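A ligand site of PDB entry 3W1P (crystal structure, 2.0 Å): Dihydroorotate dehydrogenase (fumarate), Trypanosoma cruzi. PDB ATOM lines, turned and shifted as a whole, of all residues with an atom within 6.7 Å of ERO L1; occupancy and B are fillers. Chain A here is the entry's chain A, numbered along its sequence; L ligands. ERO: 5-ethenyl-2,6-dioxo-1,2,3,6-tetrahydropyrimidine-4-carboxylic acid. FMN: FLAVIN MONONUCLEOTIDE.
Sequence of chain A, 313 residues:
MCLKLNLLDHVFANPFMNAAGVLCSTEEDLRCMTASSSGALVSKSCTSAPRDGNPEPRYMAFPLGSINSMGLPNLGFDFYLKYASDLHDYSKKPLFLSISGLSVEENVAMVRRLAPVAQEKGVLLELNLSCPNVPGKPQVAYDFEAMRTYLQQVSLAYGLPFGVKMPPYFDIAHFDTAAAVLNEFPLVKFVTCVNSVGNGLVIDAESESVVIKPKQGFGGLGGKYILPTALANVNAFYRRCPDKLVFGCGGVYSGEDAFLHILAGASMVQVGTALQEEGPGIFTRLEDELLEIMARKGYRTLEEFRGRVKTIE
The side-chain amide oxygen (OD1) of Asn 195 sits at hydrogen-bond distance from the side-chain hydroxyl (OG) of Ser 196.
The side-chain hydroxyl (OG) of Ser 130 sits at hydrogen-bond distance from the side-chain amide nitrogen (ND2) of Asn 195, at 2.8 Å.
The side-chain amide oxygen of Asn 68 is in hydrogen-bond range of the backbone NH of Met 70.
The backbone carbonyl oxygen (O) of Asn 68 sits at hydrogen-bond distance from the backbone NH (N) of Gly 220 (2.9 Å).
The backbone NH (N) of Gly 71 lies close to the side-chain amide nitrogen (ND2) of Asn 54.
O of Met 70 sits at hydrogen-bond distance from N of Asn 54 (2.8 Å).
OG of Ser 45 is in hydrogen-bond range of OG of Ser 98, at 2.5 Å.
The backbone NH of Ser 100 is in hydrogen-bond range of the backbone carbonyl oxygen of Cys 46, 2.9 Å away.
Merely in contact with ERO L1: Cys 131, Ser 45, Pro 132, Pro 73 and Ser 100.
Hydrophobic or aromatic side chains within 4 Å of ERO L1: Met 70, Leu 72, Pro 73 and Pro 132.
14 residues have an atom within 4 Å of ERO L1: Lys 44, Ser 45, Asn 68, Met 70, Gly 71, Leu 72, Pro 73, Ser 100, Asn 128, Cys 131, Pro 132, Asn 133, Asn 195 and Ser 196.
The nearest printed residue that does not touch ERO L1 is Ser 69 (4.1 Å).
An oxygen (OAE) of ERO L1 is in salt-bridge range of the side-chain amino group (NZ) of Lys 44 (2.8 Å).
A nitrogen (NAH) of ERO L1 is in hydrogen-bond range of the side-chain amide oxygen (OD1) of Asn 195, 2.8 Å away.
An oxygen (OAC) of ERO L1 lies within hydrogen-bond range of the side-chain hydroxyl (OG) of Ser 196, at 2.9 Å.
OD1 of Asn 68 sits at hydrogen-bond distance from NAG of ERO L1.
An oxygen (OAD) of ERO L1 is in hydrogen-bond range of the side-chain amide nitrogen (ND2) of Asn 128.
N of Leu 72 sits at hydrogen-bond distance from OAE of ERO L1, at 3.0 Å.
The backbone NH (N) of Gly 71 sits at hydrogen-bond distance from an oxygen (OAB) of ERO L1 (3.0 Å).
N of Met 70 sits at hydrogen-bond distance from OAB of ERO L1 (3.1 Å).
A nitrogen (NAG) of ERO L1 lies close to the side-chain amide nitrogen (ND2) of Asn 133, at 3.2 Å.
The side-chain amino group of Lys 44 lies within hydrogen-bond range of an oxygen (O4) of FMN L2.
ND2 of Asn 195 is in hydrogen-bond range of O2 of FMN L2.
The side-chain amide nitrogen (ND2) of Asn 128 is in hydrogen-bond range of an oxygen (O2) of FMN L2 (3.2 Å).
An oxygen (O4) of FMN L2 sits at hydrogen-bond distance from the backbone NH (N) of Ser 45 (3.3 Å).
The side-chain hydroxyl (OG) of Ser 45 is in hydrogen-bond range of a nitrogen (N3) of FMN L2, at 2.9 Å.
The side-chain amino group (NZ) of Lys 165 is in hydrogen-bond range of an oxygen (O2') of FMN L2 (2.8 Å).
O2' of FMN L2 lies within hydrogen-bond range of N of Ala 20 (3.5 Å).
O of Ala 20 sits close to O2' of FMN L2.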
ATOM      1  N   ALA A  20      29.883  28.431  22.773  1.00  0.00           N
ATOM      2  CA  ALA A  20      29.537  27.086  23.165  1.00  0.00           C
ATOM      3  C   ALA A  20      28.657  26.432  22.088  1.00  0.00           C
ATOM      4  O   ALA A  20      27.746  27.060  21.471  1.00  0.00           O
ATOM      5  CB  ALA A  20      28.817  27.076  24.521  1.00  0.00           C
ATOM      6  N   GLY A  21      28.916  25.166  21.902  1.00  0.00           N
ATOM      7  CA  GLY A  21      28.192  24.334  20.925  1.00  0.00           C
ATOM      8  C   GLY A  21      28.809  24.290  19.530  1.00  0.00           C
ATOM      9  O   GLY A  21      28.509  23.381  18.762  1.00  0.00           O
ATOM     10  N   LYS A  44      30.876  22.031  24.575  1.00  0.00           N
ATOM     11  CA  LYS A  44      29.442  21.959  24.288  1.00  0.00           C
ATOM     12  C   LYS A  44      28.674  21.879  25.588  1.00  0.00           C
ATOM     13  O   LYS A  44      29.049  21.078  26.470  1.00  0.00           O
ATOM     14  CB  LYS A  44      29.131  20.671  23.451  1.00  0.00           C
ATOM     15  CG  LYS A  44      27.629  20.291  23.346  1.00  0.00           C
ATOM     16  CD  LYS A  44      26.930  21.229  22.362  1.00  0.00           C
ATOM     17  CE  LYS A  44      25.421  21.224  22.486  1.00  0.00           C
ATOM     18  NZ  LYS A  44      24.740  22.200  21.551  1.00  0.00           N
ATOM     19  N   SER A  45      27.539  22.573  25.678  1.00  0.00           N
ATOM     20  CA  SER A  45      26.711  22.506  26.880  1.00  0.00           C
ATOM     21  C   SER A  45      26.308  21.078  27.107  1.00  0.00           C
ATOM     22  O   SER A  45      25.848  20.372  26.160  1.00  0.00           O
ATOM     23  CB  SER A  45      25.424  23.307  26.740  1.00  0.00           C
ATOM     24  OG  SER A  45      25.705  24.642  26.870  1.00  0.00           O
ATOM     25  N   CYS A  46      26.457  20.618  28.370  1.00  0.00           N
ATOM     26  CA  CYS A  46      26.192  19.209  28.593  1.00  0.00           C
ATOM     27  C   CYS A  46      25.064  18.936  29.601  1.00  0.00           C
ATOM     28  O   CYS A  46      24.639  19.829  30.366  1.00  0.00           O
ATOM     29  CB  CYS A  46      27.450  18.509  28.990  1.00  0.00           C
ATOM     30  SG  CYS A  46      28.050  19.068  30.590  1.00  0.00           S
ATOM     31  N   ASN A  54      18.028  16.526  18.553  1.00  0.00           N
ATOM     32  CA  ASN A  54      16.870  16.503  17.667  1.00  0.00           C
ATOM     33  C   ASN A  54      17.127  15.812  16.297  1.00  0.00           C
ATOM     34  O   ASN A  54      18.262  15.605  15.847  1.00  0.00           O
ATOM     35  CB  ASN A  54      16.308  17.948  17.459  1.00  0.00           C
ATOM     36  CG  ASN A  54      15.829  18.640  18.756  1.00  0.00           C
ATOM     37  OD1 ASN A  54      15.392  18.021  19.745  1.00  0.00           O
ATOM     38  ND2 ASN A  54      15.861  19.940  18.738  1.00  0.00           N
ATOM     39  N   ASN A  68      19.314  27.127  14.218  1.00  0.00           N
ATOM     40  CA  ASN A  68      19.552  25.782  14.707  1.00  0.00           C
ATOM     41  C   ASN A  68      18.523  25.352  15.751  1.00  0.00           C
ATOM     42  O   ASN A  68      18.035  26.172  16.510  1.00  0.00           O
ATOM     43  CB  ASN A  68      20.950  25.641  15.283  1.00  0.00           C
ATOM     44  CG  ASN A  68      21.045  26.038  16.731  1.00  0.00           C
ATOM     45  OD1 ASN A  68      20.771  25.251  17.677  1.00  0.00           O
ATOM     46  ND2 ASN A  68      21.364  27.279  16.941  1.00  0.00           N
ATOM     47  N   SER A  69      18.180  24.074  15.753  1.00  0.00           N
ATOM     48  CA  SER A  69      17.475  23.508  16.877  1.00  0.00           C
ATOM     49  C   SER A  69      18.130  22.195  17.160  1.00  0.00           C
ATOM     50  O   SER A  69      17.547  21.123  16.860  1.00  0.00           O
ATOM     51  CB  SER A  69      15.977  23.394  16.563  1.00  0.00           C
ATOM     52  OG  SER A  69      15.296  22.716  17.585  1.00  0.00           O
ATOM     53  N   MET A  70      19.368  22.277  17.684  1.00  0.00           N
ATOM     54  CA  MET A  70      20.194  21.082  17.729  1.00  0.00           C
ATOM     55  C   MET A  70      19.584  20.059  18.720  1.00  0.00           C
ATOM     56  O   MET A  70      19.662  18.832  18.531  1.00  0.00           O
ATOM     57  CB  MET A  70      21.625  21.425  18.157  1.00  0.00           C
ATOM     58  CG  MET A  70      22.377  22.396  17.305  1.00  0.00           C
ATOM     59  SD  MET A  70      22.657  21.766  15.658  1.00  0.00           S
ATOM     60  CE  MET A  70      23.940  20.535  15.910  1.00  0.00           C
ATOM     61  N   GLY A  71      18.949  20.578  19.767  1.00  0.00           N
ATOM     62  CA  GLY A  71      18.344  19.743  20.802  1.00  0.00           C
ATOM     63  C   GLY A  71      19.296  19.238  21.864  1.00  0.00           C
ATOM     64  O   GLY A  71      19.082  18.188  22.460  1.00  0.00           O
ATOM     65  N   LEU A  72      20.397  19.958  22.063  1.00  0.00           N
ATOM     66  CA  LEU A  72      21.363  19.663  23.132  1.00  0.00           C
ATOM     67  C   LEU A  72      21.995  18.287  22.997  1.00  0.00           C
ATOM     68  O   LEU A  72      22.139  17.544  23.988  1.00  0.00           O
ATOM     69  CB  LEU A  72      20.650  19.754  24.491  1.00  0.00           C
ATOM     70  CG  LEU A  72      21.322  20.702  25.475  1.00  0.00           C
ATOM     71  CD1 LEU A  72      20.575  20.701  26.818  1.00  0.00           C
ATOM     72  CD2 LEU A  72      22.823  20.427  25.613  1.00  0.00           C
ATOM     73  N   PRO A  73      22.402  17.926  21.776  1.00  0.00           N
ATOM     74  CA  PRO A  73      23.185  16.721  21.626  1.00  0.00           C
ATOM     75  C   PRO A  73      24.532  16.923  22.278  1.00  0.00           C
ATOM     76  O   PRO A  73      25.135  17.941  22.059  1.00  0.00           O
ATOM     77  CB  PRO A  73      23.386  16.590  20.101  1.00  0.00           C
ATOM     78  CG  PRO A  73      23.385  17.997  19.655  1.00  0.00           C
ATOM     79  CD  PRO A  73      22.417  18.735  20.569  1.00  0.00           C
ATOM     80  N   SER A  98      30.675  24.292  29.683  1.00  0.00           N
ATOM     81  CA  SER A  98      29.299  24.785  29.703  1.00  0.00           C
ATOM     82  C   SER A  98      28.385  23.669  30.167  1.00  0.00           C
ATOM     83  O   SER A  98      28.456  22.564  29.668  1.00  0.00           O
ATOM     84  CB  SER A  98      28.853  25.234  28.337  1.00  0.00           C
ATOM     85  OG  SER A  98      27.488  25.638  28.341  1.00  0.00           O
ATOM     86  N   SER A 100      24.241  22.649  30.903  1.00  0.00           N
ATOM     87  CA  SER A 100      22.884  23.005  30.599  1.00  0.00           C
ATOM     88  C   SER A 100      21.881  21.895  31.039  1.00  0.00           C
ATOM     89  O   SER A 100      21.106  21.360  30.226  1.00  0.00           O
ATOM     90  CB  SER A 100      22.772  23.354  29.105  1.00  0.00           C
ATOM     91  OG  SER A 100      21.551  24.062  28.911  1.00  0.00           O
ATOM     92  N   ASN A 128      24.608  27.655  31.474  1.00  0.00           N
ATOM     93  CA  ASN A 128      23.746  28.076  30.418  1.00  0.00           C
ATOM     94  C   ASN A 128      22.332  28.293  30.901  1.00  0.00           C
ATOM     95  O   ASN A 128      21.696  27.338  31.326  1.00  0.00           O
ATOM     96  CB  ASN A 128      23.771  27.030  29.307  1.00  0.00           C
ATOM     97  CG  ASN A 128      23.025  27.480  28.076  1.00  0.00           C
ATOM     98  OD1 ASN A 128      22.404  28.525  28.080  1.00  0.00           O
ATOM     99  ND2 ASN A 128      23.090  26.674  27.024  1.00  0.00           N
ATOM    100  N   SER A 130      19.929  29.765  28.899  1.00  0.00           N
ATOM    101  CA  SER A 130      19.402  30.346  27.720  1.00  0.00           C
ATOM    102  C   SER A 130      19.107  29.414  26.563  1.00  0.00           C
ATOM    103  O   SER A 130      18.897  29.898  25.476  1.00  0.00           O
ATOM    104  CB  SER A 130      20.246  31.565  27.297  1.00  0.00           C
ATOM    105  OG  SER A 130      21.591  31.314  27.240  1.00  0.00           O
ATOM    106  N   CYS A 131      19.000  28.125  26.804  1.00  0.00           N
ATOM    107  CA  CYS A 131      18.710  27.231  25.678  1.00  0.00           C
ATOM    108  C   CYS A 131      17.264  27.394  25.170  1.00  0.00           C
ATOM    109  O   CYS A 131      16.391  27.088  25.877  1.00  0.00           O
ATOM    110  CB  CYS A 131      18.977  25.799  25.991  1.00  0.00           C
ATOM    111  SG  CYS A 131      18.725  24.956  24.457  1.00  0.00           S
ATOM    112  N   PRO A 132      17.107  27.776  23.883  1.00  0.00           N
ATOM    113  CA  PRO A 132      15.785  28.074  23.285  1.00  0.00           C
ATOM    114  C   PRO A 132      15.152  26.937  22.450  1.00  0.00           C
ATOM    115  O   PRO A 132      14.079  27.191  21.855  1.00  0.00           O
ATOM    116  CB  PRO A 132      16.114  29.255  22.365  1.00  0.00           C
ATOM    117  CG  PRO A 132      17.500  28.881  21.794  1.00  0.00           C
ATOM    118  CD  PRO A 132      18.194  28.093  22.927  1.00  0.00           C
ATOM    119  N   ASN A 133      15.756  25.721  22.442  1.00  0.00           N
ATOM    120  CA  ASN A 133      15.435  24.601  21.492  1.00  0.00           C
ATOM    121  C   ASN A 133      14.934  23.216  22.024  1.00  0.00           C
ATOM    122  O   ASN A 133      14.688  22.252  21.222  1.00  0.00           O
ATOM    123  CB  ASN A 133      16.715  24.351  20.648  1.00  0.00           C
ATOM    124  CG  ASN A 133      17.074  25.567  19.817  1.00  0.00           C
ATOM    125  OD1 ASN A 133      16.172  26.277  19.327  1.00  0.00           O
ATOM    126  ND2 ASN A 133      18.372  25.833  19.652  1.00  0.00           N
ATOM    127  N   VAL A 134      14.711  23.171  23.325  1.00  0.00           N
ATOM    128  CA  VAL A 134      14.144  22.005  23.970  1.00  0.00           C
ATOM    129  C   VAL A 134      12.656  22.234  24.210  1.00  0.00           C
ATOM    130  O   VAL A 134      12.251  23.146  24.874  1.00  0.00           O
ATOM    131  CB  VAL A 134      14.848  21.628  25.254  1.00  0.00           C
ATOM    132  CG1 VAL A 134      14.131  20.423  25.883  1.00  0.00           C
ATOM    133  CG2 VAL A 134      16.310  21.329  24.982  1.00  0.00           C
ATOM    134  N   LYS A 165      25.612  32.125  30.679  1.00  0.00           N
ATOM    135  CA  LYS A 165      25.276  32.411  29.286  1.00  0.00           C
ATOM    136  C   LYS A 165      23.803  32.853  29.237  1.00  0.00           C
ATOM    137  O   LYS A 165      22.896  32.094  29.628  1.00  0.00           O
ATOM    138  CB  LYS A 165      25.505  31.191  28.416  1.00  0.00           C
ATOM    139  CG  LYS A 165      25.209  31.457  26.929  1.00  0.00           C
ATOM    140  CD  LYS A 165      26.403  32.084  26.244  1.00  0.00           C
ATOM    141  CE  LYS A 165      26.361  31.978  24.706  1.00  0.00           C
ATOM    142  NZ  LYS A 165      26.513  30.647  24.193  1.00  0.00           N
ATOM    143  N   ASN A 195      23.291  34.234  23.818  1.00  0.00           N
ATOM    144  CA  ASN A 195      22.821  33.034  23.167  1.00  0.00           C
ATOM    145  C   ASN A 195      22.020  33.442  21.914  1.00  0.00           C
ATOM    146  O   ASN A 195      21.838  34.656  21.624  1.00  0.00           O
ATOM    147  CB  ASN A 195      21.996  32.169  24.150  1.00  0.00           C
ATOM    148  CG  ASN A 195      22.139  30.650  23.875  1.00  0.00           C
ATOM    149  OD1 ASN A 195      22.011  30.200  22.722  1.00  0.00           O
ATOM    150  ND2 ASN A 195      22.350  29.877  24.933  1.00  0.00           N
ATOM    151  N   SER A 196      21.654  32.449  21.124  1.00  0.00           N
ATOM    152  CA  SER A 196      20.931  32.690  19.883  1.00  0.00           C
ATOM    153  C   SER A 196      19.640  33.425  20.111  1.00  0.00           C
ATOM    154  O   SER A 196      19.020  33.377  21.243  1.00  0.00           O
ATOM    155  CB  SER A 196      20.788  31.329  19.118  1.00  0.00           C
ATOM    156  OG  SER A 196      20.061  30.398  19.838  1.00  0.00           O
ATOM    157  N   GLY A 220      16.940  28.804  16.937  1.00  0.00           N
ATOM    158  CA  GLY A 220      17.713  29.940  17.345  1.00  0.00           C
ATOM    159  C   GLY A 220      18.517  30.573  16.202  1.00  0.00           C
ATOM    160  O   GLY A 220      19.234  29.865  15.498  1.00  0.00           O
ATOM    161  N   LEU A 221      18.499  31.913  16.127  1.00  0.00           N
ATOM    162  CA  LEU A 221      19.226  32.643  15.123  1.00  0.00           C
ATOM    163  C   LEU A 221      20.593  33.118  15.621  1.00  0.00           C
ATOM    164  O   LEU A 221      20.775  33.631  16.775  1.00  0.00           O
ATOM    165  CB  LEU A 221      18.416  33.810  14.651  1.00  0.00           C
ATOM    166  CG  LEU A 221      16.973  33.539  14.179  1.00  0.00           C
ATOM    167  CD1 LEU A 221      16.251  34.847  13.916  1.00  0.00           C
ATOM    168  CD2 LEU A 221      17.043  32.697  12.931  1.00  0.00           C
HETATM  169  OAB ERO L   1      20.204  23.238  20.513  1.00  0.00           O
HETATM  170  CAI ERO L   1      21.297  23.424  21.153  1.00  0.00           C
HETATM  171  OAE ERO L   1      21.933  22.491  21.579  1.00  0.00           O
HETATM  172  CAK ERO L   1      21.553  24.751  21.520  1.00  0.00           C
HETATM  173  NAG ERO L   1      21.461  25.669  20.507  1.00  0.00           N
HETATM  174  CAL ERO L   1      21.597  27.014  20.800  1.00  0.00           C
HETATM  175  OAC ERO L   1      21.550  27.876  19.918  1.00  0.00           O
HETATM  176  NAH ERO L   1      21.758  27.435  22.104  1.00  0.00           N
HETATM  177  CAM ERO L   1      21.816  26.531  23.157  1.00  0.00           C
HETATM  178  OAD ERO L   1      21.934  27.002  24.284  1.00  0.00           O
HETATM  179  CAJ ERO L   1      21.677  25.166  22.872  1.00  0.00           C
HETATM  180  CAF ERO L   1      21.681  24.190  23.901  1.00  0.00           C
HETATM  181  CAA ERO L   1      22.545  24.324  25.074  1.00  0.00           C
HETATM  182  N1  FMN L   2      25.092  28.031  23.100  1.00  0.00           N
HETATM  183  C2  FMN L   2      25.275  27.439  24.265  1.00  0.00           C
HETATM  184  O2  FMN L   2      25.336  28.141  25.340  1.00  0.00           O
HETATM  185  N3  FMN L   2      25.426  26.107  24.344  1.00  0.00           N
HETATM  186  C4  FMN L   2      25.381  25.261  23.331  1.00  0.00           C
HETATM  187  O4  FMN L   2      25.574  24.016  23.498  1.00  0.00           O
HETATM  188  C4A FMN L   2      25.169  25.832  22.012  1.00  0.00           C
HETATM  189  N5  FMN L   2      25.144  25.086  20.872  1.00  0.00           N
HETATM  190  C5A FMN L   2      25.081  25.709  19.672  1.00  0.00           C
HETATM  191  C6  FMN L   2      25.089  24.957  18.515  1.00  0.00           C
HETATM  192  C7  FMN L   2      25.010  25.501  17.265  1.00  0.00           C
HETATM  193  C7M FMN L   2      25.055  24.593  16.066  1.00  0.00           C
HETATM  194  C8  FMN L   2      24.914  26.969  17.161  1.00  0.00           C
HETATM  195  C8M FMN L   2      24.789  27.646  15.843  1.00  0.00           C
HETATM  196  C9  FMN L   2      24.872  27.758  18.338  1.00  0.00           C
HETATM  197  C9A FMN L   2      24.926  27.182  19.572  1.00  0.00           C
HETATM  198  N10 FMN L   2      24.839  27.910  20.730  1.00  0.00           N
HETATM  199  C10 FMN L   2      25.021  27.303  21.960  1.00  0.00           C
HETATM  200  C1' FMN L   2      24.756  29.354  20.687  1.00  0.00           C
HETATM  201  C2' FMN L   2      26.120  29.982  20.425  1.00  0.00           C
HETATM  202  O2' FMN L   2      26.919  29.744  21.547  1.00  0.00           O
HETATM  203  C3' FMN L   2      25.947  31.480  20.250  1.00  0.00           C
HETATM  204  O3' FMN L   2      25.464  32.066  21.476  1.00  0.00           O
HETATM  205  C4' FMN L   2      25.007  31.911  19.106  1.00  0.00           C
HETATM  206  O4' FMN L   2      25.258  31.063  17.967  1.00  0.00           O
HETATM  207  C5' FMN L   2      25.202  33.378  18.715  1.00  0.00           C
HETATM  208  O5' FMN L   2      26.516  33.638  18.204  1.00  0.00           O
HETATM  209  P   FMN L   2      26.913  33.704  16.623  1.00  0.00           P
HETATM  210  O1P FMN L   2      28.386  33.902  16.580  1.00  0.00           O
HETATM  211  O2P FMN L   2      26.109  34.874  16.098  1.00  0.00           O
HETATM  212  O3P FMN L   2      26.430  32.376  16.066  1.00  0.00           O
